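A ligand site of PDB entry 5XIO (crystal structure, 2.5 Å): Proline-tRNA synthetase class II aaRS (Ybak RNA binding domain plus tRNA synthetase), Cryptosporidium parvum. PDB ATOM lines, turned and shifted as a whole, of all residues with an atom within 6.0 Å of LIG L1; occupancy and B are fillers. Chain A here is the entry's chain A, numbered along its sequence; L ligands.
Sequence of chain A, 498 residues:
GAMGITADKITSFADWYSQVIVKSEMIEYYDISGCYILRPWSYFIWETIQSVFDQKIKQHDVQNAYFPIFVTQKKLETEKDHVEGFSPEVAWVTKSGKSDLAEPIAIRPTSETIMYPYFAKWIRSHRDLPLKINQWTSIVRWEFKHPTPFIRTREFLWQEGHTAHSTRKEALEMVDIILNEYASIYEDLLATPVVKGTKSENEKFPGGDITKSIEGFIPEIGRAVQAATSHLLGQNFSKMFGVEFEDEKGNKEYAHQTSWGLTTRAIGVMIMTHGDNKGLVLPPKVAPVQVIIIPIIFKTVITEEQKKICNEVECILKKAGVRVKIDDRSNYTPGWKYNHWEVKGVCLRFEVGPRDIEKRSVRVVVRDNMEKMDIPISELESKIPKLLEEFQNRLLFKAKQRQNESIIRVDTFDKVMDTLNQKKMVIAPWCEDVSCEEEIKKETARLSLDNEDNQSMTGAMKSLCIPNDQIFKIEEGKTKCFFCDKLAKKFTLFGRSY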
ATOM      1  N   LEU A  76      -0.450 -12.983   0.884  1.00  0.00           N
ATOM      2  CA  LEU A  76      -1.049 -11.644   0.851  1.00  0.00           C
ATOM      3  C   LEU A  76      -2.339 -11.707   0.059  1.00  0.00           C
ATOM      4  O   LEU A  76      -3.312 -11.033   0.415  1.00  0.00           O
ATOM      5  CB  LEU A  76      -0.074 -10.603   0.251  1.00  0.00           C
ATOM      6  CG  LEU A  76      -0.517  -9.145   0.221  1.00  0.00           C
ATOM      7  CD1 LEU A  76      -0.757  -8.634   1.637  1.00  0.00           C
ATOM      8  CD2 LEU A  76       0.489  -8.224  -0.472  1.00  0.00           C
ATOM      9  N   PHE A  86      -7.362  -4.585  -2.439  1.00  0.00           N
ATOM     10  CA  PHE A  86      -6.459  -3.536  -1.918  1.00  0.00           C
ATOM     11  C   PHE A  86      -5.110  -3.384  -2.673  1.00  0.00           C
ATOM     12  O   PHE A  86      -4.385  -2.403  -2.416  1.00  0.00           O
ATOM     13  CB  PHE A  86      -6.200  -3.757  -0.406  1.00  0.00           C
ATOM     14  CG  PHE A  86      -7.074  -2.916   0.507  1.00  0.00           C
ATOM     15  CD1 PHE A  86      -7.012  -1.499   0.463  1.00  0.00           C
ATOM     16  CD2 PHE A  86      -7.933  -3.513   1.441  1.00  0.00           C
ATOM     17  CE1 PHE A  86      -7.798  -0.727   1.312  1.00  0.00           C
ATOM     18  CE2 PHE A  86      -8.719  -2.741   2.290  1.00  0.00           C
ATOM     19  CZ  PHE A  86      -8.659  -1.339   2.229  1.00  0.00           C
ATOM     20  N   SER A  87      -4.817  -4.270  -3.634  1.00  0.00           N
ATOM     21  CA  SER A  87      -3.436  -4.534  -4.171  1.00  0.00           C
ATOM     22  C   SER A  87      -2.579  -3.408  -4.907  1.00  0.00           C
ATOM     23  O   SER A  87      -1.354  -3.445  -4.791  1.00  0.00           O
ATOM     24  CB  SER A  87      -3.411  -5.870  -5.001  1.00  0.00           C
ATOM     25  N   PRO A  88      -3.210  -2.421  -5.615  1.00  0.00           N
ATOM     26  CA  PRO A  88      -2.405  -1.392  -6.379  1.00  0.00           C
ATOM     27  C   PRO A  88      -1.455  -0.444  -5.584  1.00  0.00           C
ATOM     28  O   PRO A  88      -0.704   0.334  -6.204  1.00  0.00           O
ATOM     29  CB  PRO A  88      -3.480  -0.528  -7.081  1.00  0.00           C
ATOM     30  CG  PRO A  88      -4.823  -1.096  -6.727  1.00  0.00           C
ATOM     31  CD  PRO A  88      -4.653  -2.078  -5.603  1.00  0.00           C
ATOM     32  N   GLU A  89      -1.505  -0.471  -4.259  1.00  0.00           N
ATOM     33  CA  GLU A  89      -0.727   0.443  -3.448  1.00  0.00           C
ATOM     34  C   GLU A  89       0.383  -0.338  -2.715  1.00  0.00           C
ATOM     35  O   GLU A  89       1.098   0.230  -1.900  1.00  0.00           O
ATOM     36  CB  GLU A  89      -1.628   1.254  -2.475  1.00  0.00           C
ATOM     37  CG  GLU A  89      -3.093   1.357  -2.847  1.00  0.00           C
ATOM     38  CD  GLU A  89      -3.774   2.595  -2.258  1.00  0.00           C
ATOM     39  OE1 GLU A  89      -3.550   2.912  -1.046  1.00  0.00           O
ATOM     40  OE2 GLU A  89      -4.568   3.229  -3.044  1.00  0.00           O
ATOM     41  N   VAL A  90       0.557  -1.624  -3.040  1.00  0.00           N
ATOM     42  CA  VAL A  90       1.570  -2.473  -2.414  1.00  0.00           C
ATOM     43  C   VAL A  90       2.905  -2.385  -3.133  1.00  0.00           C
ATOM     44  O   VAL A  90       2.955  -2.547  -4.339  1.00  0.00           O
ATOM     45  CB  VAL A  90       1.140  -3.951  -2.400  1.00  0.00           C
ATOM     46  CG1 VAL A  90       2.219  -4.820  -1.758  1.00  0.00           C
ATOM     47  CG2 VAL A  90      -0.133  -4.130  -1.648  1.00  0.00           C
ATOM     48  N   PRO A 109       2.017  -3.923   4.335  1.00  0.00           N
ATOM     49  CA  PRO A 109       1.083  -2.814   4.346  1.00  0.00           C
ATOM     50  C   PRO A 109       0.200  -2.798   5.569  1.00  0.00           C
ATOM     51  O   PRO A 109      -0.374  -1.813   5.821  1.00  0.00           O
ATOM     52  CB  PRO A 109       0.246  -3.099   3.129  1.00  0.00           C
ATOM     53  CG  PRO A 109       0.207  -4.544   3.047  1.00  0.00           C
ATOM     54  CD  PRO A 109       1.525  -5.029   3.513  1.00  0.00           C
ATOM     55  N   THR A 110       0.148  -3.907   6.258  1.00  0.00           N
ATOM     56  CA  THR A 110      -0.583  -4.263   7.473  1.00  0.00           C
ATOM     57  C   THR A 110      -0.235  -5.747   7.745  1.00  0.00           C
ATOM     58  O   THR A 110       0.103  -6.475   6.869  1.00  0.00           O
ATOM     59  CB  THR A 110      -2.107  -3.969   7.393  1.00  0.00           C
ATOM     60  OG1 THR A 110      -2.707  -4.111   8.648  1.00  0.00           O
ATOM     61  CG2 THR A 110      -2.755  -4.772   6.380  1.00  0.00           C
ATOM     62  N   SER A 111      -0.375  -6.166   8.983  1.00  0.00           N
ATOM     63  CA  SER A 111       0.043  -7.473   9.366  1.00  0.00           C
ATOM     64  C   SER A 111      -0.892  -8.646   9.536  1.00  0.00           C
ATOM     65  O   SER A 111      -0.463  -9.649   9.977  1.00  0.00           O
ATOM     66  CB  SER A 111       0.875  -7.323  10.605  1.00  0.00           C
ATOM     67  OG  SER A 111       2.111  -6.933  10.212  1.00  0.00           O
ATOM     68  N   GLU A 112      -2.135  -8.557   9.118  1.00  0.00           N
ATOM     69  CA  GLU A 112      -3.086  -9.651   9.278  1.00  0.00           C
ATOM     70  C   GLU A 112      -2.699 -10.959   8.640  1.00  0.00           C
ATOM     71  O   GLU A 112      -2.873 -11.986   9.215  1.00  0.00           O
ATOM     72  CB  GLU A 112      -4.435  -9.258   8.701  1.00  0.00           C
ATOM     73  CG  GLU A 112      -5.284  -8.412   9.583  1.00  0.00           C
ATOM     74  CD  GLU A 112      -4.970  -6.937   9.433  1.00  0.00           C
ATOM     75  OE1 GLU A 112      -4.162  -6.585   8.622  1.00  0.00           O
ATOM     76  OE2 GLU A 112      -5.554  -6.142  10.135  1.00  0.00           O
ATOM     77  N   VAL A 140       4.651   0.683   4.768  1.00  0.00           N
ATOM     78  CA  VAL A 140       4.680   1.286   3.453  1.00  0.00           C
ATOM     79  C   VAL A 140       3.426   1.057   2.702  1.00  0.00           C
ATOM     80  O   VAL A 140       2.940  -0.073   2.629  1.00  0.00           O
ATOM     81  CB  VAL A 140       5.802   0.701   2.611  1.00  0.00           C
ATOM     82  CG1 VAL A 140       5.740   1.252   1.174  1.00  0.00           C
ATOM     83  CG2 VAL A 140       7.147   1.012   3.250  1.00  0.00           C
ATOM     84  N   ARG A 141       2.917   2.128   2.109  1.00  0.00           N
ATOM     85  CA  ARG A 141       1.768   2.064   1.164  1.00  0.00           C
ATOM     86  C   ARG A 141       1.946   3.048   0.064  1.00  0.00           C
ATOM     87  O   ARG A 141       2.250   4.216   0.290  1.00  0.00           O
ATOM     88  CB  ARG A 141       0.449   2.366   1.857  1.00  0.00           C
ATOM     89  CG  ARG A 141       0.019   1.291   2.843  1.00  0.00           C
ATOM     90  CD  ARG A 141      -1.198   1.730   3.616  1.00  0.00           C
ATOM     91  NE  ARG A 141      -1.448   0.898   4.791  1.00  0.00           N
ATOM     92  CZ  ARG A 141      -2.454   1.110   5.654  1.00  0.00           C
ATOM     93  NH1 ARG A 141      -3.260   2.145   5.510  1.00  0.00           N
ATOM     94  NH2 ARG A 141      -2.664   0.291   6.671  1.00  0.00           N
ATOM     95  N   TRP A 142       1.765   2.605  -1.157  1.00  0.00           N
ATOM     96  CA  TRP A 142       2.034   3.470  -2.299  1.00  0.00           C
ATOM     97  C   TRP A 142       0.801   4.304  -2.552  1.00  0.00           C
ATOM     98  O   TRP A 142      -0.033   3.894  -3.345  1.00  0.00           O
ATOM     99  CB  TRP A 142       2.373   2.671  -3.548  1.00  0.00           C
ATOM    100  CG  TRP A 142       3.491   3.279  -4.286  1.00  0.00           C
ATOM    101  CD1 TRP A 142       3.443   4.051  -5.428  1.00  0.00           C
ATOM    102  CD2 TRP A 142       4.849   3.207  -3.902  1.00  0.00           C
ATOM    103  NE1 TRP A 142       4.690   4.428  -5.766  1.00  0.00           N
ATOM    104  CE2 TRP A 142       5.582   3.931  -4.859  1.00  0.00           C
ATOM    105  CE3 TRP A 142       5.526   2.584  -2.842  1.00  0.00           C
ATOM    106  CZ2 TRP A 142       6.964   4.065  -4.794  1.00  0.00           C
ATOM    107  CZ3 TRP A 142       6.895   2.714  -2.767  1.00  0.00           C
ATOM    108  CH2 TRP A 142       7.603   3.452  -3.747  1.00  0.00           C
ATOM    109  N   TRP A 158       3.664   3.294  13.103  1.00  0.00           N
ATOM    110  CA  TRP A 158       2.434   3.032  13.887  1.00  0.00           C
ATOM    111  C   TRP A 158       2.579   1.956  14.952  1.00  0.00           C
ATOM    112  O   TRP A 158       3.635   1.318  15.082  1.00  0.00           O
ATOM    113  CB  TRP A 158       1.280   2.663  12.936  1.00  0.00           C
ATOM    114  CG  TRP A 158       1.193   1.206  12.423  1.00  0.00           C
ATOM    115  CD1 TRP A 158       2.100   0.183  12.545  1.00  0.00           C
ATOM    116  CD2 TRP A 158       0.107   0.651  11.653  1.00  0.00           C
ATOM    117  NE1 TRP A 158       1.666  -0.963  11.868  1.00  0.00           N
ATOM    118  CE2 TRP A 158       0.439  -0.700  11.335  1.00  0.00           C
ATOM    119  CE3 TRP A 158      -1.087   1.187  11.176  1.00  0.00           C
ATOM    120  CZ2 TRP A 158      -0.377  -1.517  10.603  1.00  0.00           C
ATOM    121  CZ3 TRP A 158      -1.900   0.383  10.450  1.00  0.00           C
ATOM    122  CH2 TRP A 158      -1.557  -0.986  10.168  1.00  0.00           C
ATOM    123  N   GLN A 159       1.539   1.751  15.713  1.00  0.00           N
ATOM    124  CA  GLN A 159       1.356   0.467  16.383  1.00  0.00           C
ATOM    125  C   GLN A 159       0.141  -0.214  15.756  1.00  0.00           C
ATOM    126  O   GLN A 159      -0.733   0.461  15.289  1.00  0.00           O
ATOM    127  CB  GLN A 159       1.238   0.582  17.920  1.00  0.00           C
ATOM    128  CG  GLN A 159       0.171   1.551  18.408  1.00  0.00           C
ATOM    129  CD  GLN A 159      -1.224   1.058  18.330  1.00  0.00           C
ATOM    130  OE1 GLN A 159      -2.141   1.878  18.166  1.00  0.00           O
ATOM    131  NE2 GLN A 159      -1.446  -0.285  18.529  1.00  0.00           N
ATOM    132  N   GLU A 160       0.137  -1.546  15.698  1.00  0.00           N
ATOM    133  CA  GLU A 160      -1.076  -2.296  15.367  1.00  0.00           C
ATOM    134  C   GLU A 160      -1.301  -3.331  16.458  1.00  0.00           C
ATOM    135  O   GLU A 160      -0.381  -4.110  16.746  1.00  0.00           O
ATOM    136  CB  GLU A 160      -0.953  -3.006  14.031  1.00  0.00           C
ATOM    137  CG  GLU A 160       0.364  -3.687  13.700  1.00  0.00           C
ATOM    138  CD  GLU A 160       0.301  -4.328  12.334  1.00  0.00           C
ATOM    139  OE1 GLU A 160      -0.792  -4.869  11.921  1.00  0.00           O
ATOM    140  OE2 GLU A 160       1.348  -4.341  11.627  1.00  0.00           O
ATOM    141  N   GLY A 161      -2.482  -3.303  17.077  1.00  0.00           N
ATOM    142  CA  GLY A 161      -2.858  -4.271  18.089  1.00  0.00           C
ATOM    143  C   GLY A 161      -3.832  -5.313  17.452  1.00  0.00           C
ATOM    144  O   GLY A 161      -4.675  -4.933  16.626  1.00  0.00           O
ATOM    145  N   HIS A 162      -3.727  -6.565  17.870  1.00  0.00           N
ATOM    146  CA  HIS A 162      -4.466  -7.711  17.282  1.00  0.00           C
ATOM    147  C   HIS A 162      -4.833  -8.644  18.450  1.00  0.00           C
ATOM    148  O   HIS A 162      -3.929  -9.222  19.047  1.00  0.00           O
ATOM    149  CB  HIS A 162      -3.570  -8.477  16.308  1.00  0.00           C
ATOM    150  CG  HIS A 162      -3.178  -7.707  15.089  1.00  0.00           C
ATOM    151  ND1 HIS A 162      -3.953  -7.656  13.955  1.00  0.00           N
ATOM    152  CD2 HIS A 162      -2.106  -6.906  14.849  1.00  0.00           C
ATOM    153  CE1 HIS A 162      -3.385  -6.868  13.063  1.00  0.00           C
ATOM    154  NE2 HIS A 162      -2.246  -6.419  13.571  1.00  0.00           N
ATOM    155  N   PHE A 205     -14.170  -1.023   7.583  1.00  0.00           N
ATOM    156  CA  PHE A 205     -13.166  -1.955   7.106  1.00  0.00           C
ATOM    157  C   PHE A 205     -13.844  -3.233   6.645  1.00  0.00           C
ATOM    158  O   PHE A 205     -14.545  -3.883   7.418  1.00  0.00           O
ATOM    159  CB  PHE A 205     -12.193  -2.273   8.238  1.00  0.00           C
ATOM    160  CG  PHE A 205     -11.176  -3.313   7.921  1.00  0.00           C
ATOM    161  CD1 PHE A 205     -10.560  -3.363   6.704  1.00  0.00           C
ATOM    162  CD2 PHE A 205     -10.804  -4.206   8.902  1.00  0.00           C
ATOM    163  CE1 PHE A 205      -9.586  -4.335   6.422  1.00  0.00           C
ATOM    164  CE2 PHE A 205      -9.809  -5.165   8.658  1.00  0.00           C
ATOM    165  CZ  PHE A 205      -9.214  -5.229   7.402  1.00  0.00           C
ATOM    166  N   THR A 229      -8.475   4.109  14.661  1.00  0.00           N
ATOM    167  CA  THR A 229      -9.648   3.186  14.529  1.00  0.00           C
ATOM    168  C   THR A 229      -9.469   1.860  15.244  1.00  0.00           C
ATOM    169  O   THR A 229      -8.331   1.448  15.524  1.00  0.00           O
ATOM    170  CB  THR A 229      -9.873   2.766  13.074  1.00  0.00           C
ATOM    171  OG1 THR A 229      -8.609   2.727  12.439  1.00  0.00           O
ATOM    172  CG2 THR A 229     -10.763   3.730  12.339  1.00  0.00           C
ATOM    173  N   HIS A 231     -11.391  -2.062  15.389  1.00  0.00           N
ATOM    174  CA  HIS A 231     -12.377  -2.972  14.781  1.00  0.00           C
ATOM    175  C   HIS A 231     -12.753  -4.197  15.681  1.00  0.00           C
ATOM    176  O   HIS A 231     -11.887  -4.844  16.338  1.00  0.00           O
ATOM    177  CB  HIS A 231     -11.821  -3.574  13.495  1.00  0.00           C
ATOM    178  CG  HIS A 231     -11.178  -2.599  12.588  1.00  0.00           C
ATOM    179  ND1 HIS A 231     -11.891  -1.718  11.813  1.00  0.00           N
ATOM    180  CD2 HIS A 231      -9.876  -2.356  12.315  1.00  0.00           C
ATOM    181  CE1 HIS A 231     -11.063  -0.989  11.104  1.00  0.00           C
ATOM    182  NE2 HIS A 231      -9.836  -1.359  11.375  1.00  0.00           N
ATOM    183  N   SER A 259      -8.887  -5.683  16.117  1.00  0.00           N
ATOM    184  CA  SER A 259      -7.665  -5.013  15.736  1.00  0.00           C
ATOM    185  C   SER A 259      -7.818  -3.525  15.764  1.00  0.00           C
ATOM    186  O   SER A 259      -8.923  -3.015  15.707  1.00  0.00           O
ATOM    187  CB  SER A 259      -7.139  -5.495  14.409  1.00  0.00           C
ATOM    188  OG  SER A 259      -7.787  -4.886  13.332  1.00  0.00           O
ATOM    189  N   TRP A 260      -6.704  -2.815  15.877  1.00  0.00           N
ATOM    190  CA  TRP A 260      -6.689  -1.365  16.123  1.00  0.00           C
ATOM    191  C   TRP A 260      -5.266  -0.813  15.774  1.00  0.00           C
ATOM    192  O   TRP A 260      -4.234  -1.503  15.968  1.00  0.00           O
ATOM    193  CB  TRP A 260      -7.000  -1.085  17.606  1.00  0.00           C
ATOM    194  CG  TRP A 260      -6.807  -2.233  18.576  1.00  0.00           C
ATOM    195  CD1 TRP A 260      -7.631  -3.295  18.740  1.00  0.00           C
ATOM    196  CD2 TRP A 260      -5.720  -2.430  19.482  1.00  0.00           C
ATOM    197  NE1 TRP A 260      -7.135  -4.139  19.699  1.00  0.00           N
ATOM    198  CE2 TRP A 260      -5.963  -3.638  20.153  1.00  0.00           C
ATOM    199  CE3 TRP A 260      -4.567  -1.703  19.808  1.00  0.00           C
ATOM    200  CZ2 TRP A 260      -5.120  -4.126  21.161  1.00  0.00           C
ATOM    201  CZ3 TRP A 260      -3.699  -2.216  20.792  1.00  0.00           C
ATOM    202  CH2 TRP A 260      -3.983  -3.393  21.444  1.00  0.00           C
ATOM    203  N   GLY A 261      -5.237   0.443  15.295  1.00  0.00           N
ATOM    204  CA  GLY A 261      -3.958   1.165  14.943  1.00  0.00           C
ATOM    205  C   GLY A 261      -3.999   2.680  15.110  1.00  0.00           C
ATOM    206  O   GLY A 261      -5.045   3.315  14.980  1.00  0.00           O
HETATM  207  O1  LIG L   1      -5.048  -1.882   7.900  1.00  0.00           O
HETATM  208  C1  LIG L   1      -6.235  -2.096   7.837  1.00  0.00           C
HETATM  209  C2  LIG L   1      -7.026  -2.722   8.974  1.00  0.00           C
HETATM  210  C3  LIG L   1      -6.284  -2.622  10.319  1.00  0.00           C
HETATM  211  N1  LIG L   1      -5.112  -3.474  10.369  1.00  0.00           N
HETATM  212  C4  LIG L   1      -4.548  -3.497  11.711  1.00  0.00           C
HETATM  213  C5  LIG L   1      -4.205  -2.103  12.201  1.00  0.00           C
HETATM  214  C6  LIG L   1      -5.397  -1.175  12.080  1.00  0.00           C
HETATM  215  C7  LIG L   1      -5.926  -1.193  10.666  1.00  0.00           C
HETATM  216  O2  LIG L   1      -7.060  -0.364  10.580  1.00  0.00           O
HETATM  217  C8  LIG L   1      -7.047  -1.778   6.583  1.00  0.00           C
HETATM  218  N2  LIG L   1      -6.155  -1.617   5.429  1.00  0.00           N
HETATM  219  C9  LIG L   1      -5.766  -2.746   4.727  1.00  0.00           C
HETATM  220  O3  LIG L   1      -6.102  -3.849   5.071  1.00  0.00           O
HETATM  221  C10 LIG L   1      -4.863  -2.481   3.609  1.00  0.00           C
HETATM  222  C11 LIG L   1      -4.378  -3.531   2.835  1.00  0.00           C
HETATM  223  C12 LIG L   1      -5.763  -0.393   5.035  1.00  0.00           C
HETATM  224  N3  LIG L   1      -4.989  -0.124   4.059  1.00  0.00           N
HETATM  225  C13 LIG L   1      -4.507  -1.178   3.307  1.00  0.00           C
HETATM  226  C14 LIG L   1      -3.666  -0.923   2.242  1.00  0.00           C
HETATM  227  C15 LIG L   1      -3.161  -1.951   1.454  1.00  0.00           C
HETATM  228 BR1  LIG L   1      -1.984  -1.519   0.039  1.00  0.00          BR
HETATM  229  C16 LIG L   1      -3.523  -3.269   1.769  1.00  0.00           C
HETATM  230 CL1  LIG L   1      -2.949  -4.576   0.835  1.00  0.00          CL
HETATM  231  P1  LG2 L   2      -7.557   6.232   5.584  1.00  0.00           P
HETATM  232  O1  LG2 L   2      -7.622   7.418   6.410  1.00  0.00           O
HETATM  233  O2  LG2 L   2      -8.380   6.412   4.282  1.00  0.00           O
HETATM  234  O3  LG2 L   2      -6.112   5.965   5.130  1.00  0.00           O
HETATM  235  P2  LG2 L   2      -7.538   3.573   6.095  1.00  0.00           P
HETATM  236  O4  LG2 L   2      -6.734   3.522   4.797  1.00  0.00           O
HETATM  237  O5  LG2 L   2      -8.469   2.487   6.181  1.00  0.00           O
HETATM  238  N1  LG2 L   2      -8.149   4.995   6.474  1.00  0.00           N
HETATM  239  P3  LG2 L   2      -6.283   2.163   8.338  1.00  0.00           P
HETATM  240  O6  LG2 L   2      -5.616   1.062   7.703  1.00  0.00           O
HETATM  241  O7  LG2 L   2      -7.533   1.902   9.008  1.00  0.00           O
HETATM  242  O8  LG2 L   2      -6.484   3.321   7.262  1.00  0.00           O
HETATM  243  O9  LG2 L   2      -5.259   2.820   9.339  1.00  0.00           O
HETATM  244  C1  LG2 L   2      -5.670   3.369  10.579  1.00  0.00           C
HETATM  245  C2  LG2 L   2      -5.080   4.764  10.814  1.00  0.00           C
HETATM  246  O10 LG2 L   2      -3.864   4.971  10.095  1.00  0.00           O
HETATM  247  C3  LG2 L   2      -6.056   5.709  10.143  1.00  0.00           C
HETATM  248  O11 LG2 L   2      -7.173   5.975  11.023  1.00  0.00           O
HETATM  249  C4  LG2 L   2      -5.236   6.955   9.882  1.00  0.00           C
HETATM  250  O12 LG2 L   2      -5.247   7.847  11.009  1.00  0.00           O
HETATM  251  C5  LG2 L   2      -3.825   6.383   9.732  1.00  0.00           C
HETATM  252  N2  LG2 L   2      -3.329   6.462   8.336  1.00  0.00           N
HETATM  253  C6  LG2 L   2      -3.826   5.804   7.248  1.00  0.00           C
HETATM  254  N3  LG2 L   2      -3.145   6.004   6.123  1.00  0.00           N
HETATM  255  C7  LG2 L   2      -2.110   6.819   6.549  1.00  0.00           C
HETATM  256  C8  LG2 L   2      -1.018   7.399   5.880  1.00  0.00           C
HETATM  257  N4  LG2 L   2      -0.822   7.236   4.573  1.00  0.00           N
HETATM  258  N5  LG2 L   2      -0.160   8.164   6.554  1.00  0.00           N
HETATM  259  C9  LG2 L   2      -0.350   8.343   7.847  1.00  0.00           C
HETATM  260  N6  LG2 L   2      -1.344   7.855   8.587  1.00  0.00           N
HETATM  261  C10 LG2 L   2      -2.201   7.087   7.904  1.00  0.00           C
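Merely in contact with LIG L1: Phe 86 (3.5 Å), Trp 158 (3.5 Å), Gly 261 (3.6 Å), Phe 205 (3.6 Å), Val 90 (3.6 Å), Trp 260 (3.7 Å), Glu 89 (3.8 Å), His 162 (3.8 Å), Glu 160 (3.8 Å), Pro 109 (3.9 Å), Ser 259 (3.9 Å) and Thr 229 (3.9 Å). Hydrophobic or aromatic side chains that line LIG L1: Phe 86, Val 90, Pro 109, Trp 158, His 162, Phe 205 and His 231. Of the 24 residues printed, 16 come within 4 Å of LIG L1.
OE2 of Glu 160 sits at hydrogen-bond distance from NE1 of Trp 158, at 3.4 Å. The backbone NH of His 231 is in hydrogen-bond range of the backbone carbonyl oxygen of Ser 259, 2.7 Å away. OE1 of Glu 112 is in hydrogen-bond range of OG1 of Thr 110. The backbone NH (N) of Gly 261 sits at hydrogen-bond distance from the backbone carbonyl oxygen (O) of Thr 229 (3.3 Å). The backbone NH (N) of Gly 161 is in hydrogen-bond range of the backbone carbonyl oxygen (O) of Trp 260. The side-chain carboxylate (OE1) of Glu 160 sits at hydrogen-bond distance from a ring nitrogen (NE2) of His 162 (2.7 Å). The backbone carbonyl oxygen (O) of Pro 109 lies within hydrogen-bond range of the guanidinium group (NE) of Arg 141 (3.1 Å). OE2 of Glu 160 sits at hydrogen-bond distance from OG of Ser 111 (3.1 Å).
An oxygen (O7) of LG2 L2 lies within hydrogen-bond range of an oxygen (O2) of LIG L1 (2.8 Å).
The side-chain hydroxyl (OG1) of Thr 110 is in hydrogen-bond range of a nitrogen (N1) of LIG L1 (3.0 Å). OE2 of Glu 112 lies within salt-bridge range of N1 of LIG L1 (2.7 Å). N3 of LIG L1 is in hydrogen-bond range of NH1 of Arg 141. A ring nitrogen (NE2) of His 231 lies within hydrogen-bond range of an oxygen (O2) of LIG L1 (3.1 Å). An oxygen (O6) of LG2 L2 is in salt-bridge range of the guanidinium group (NH2) of Arg 141.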
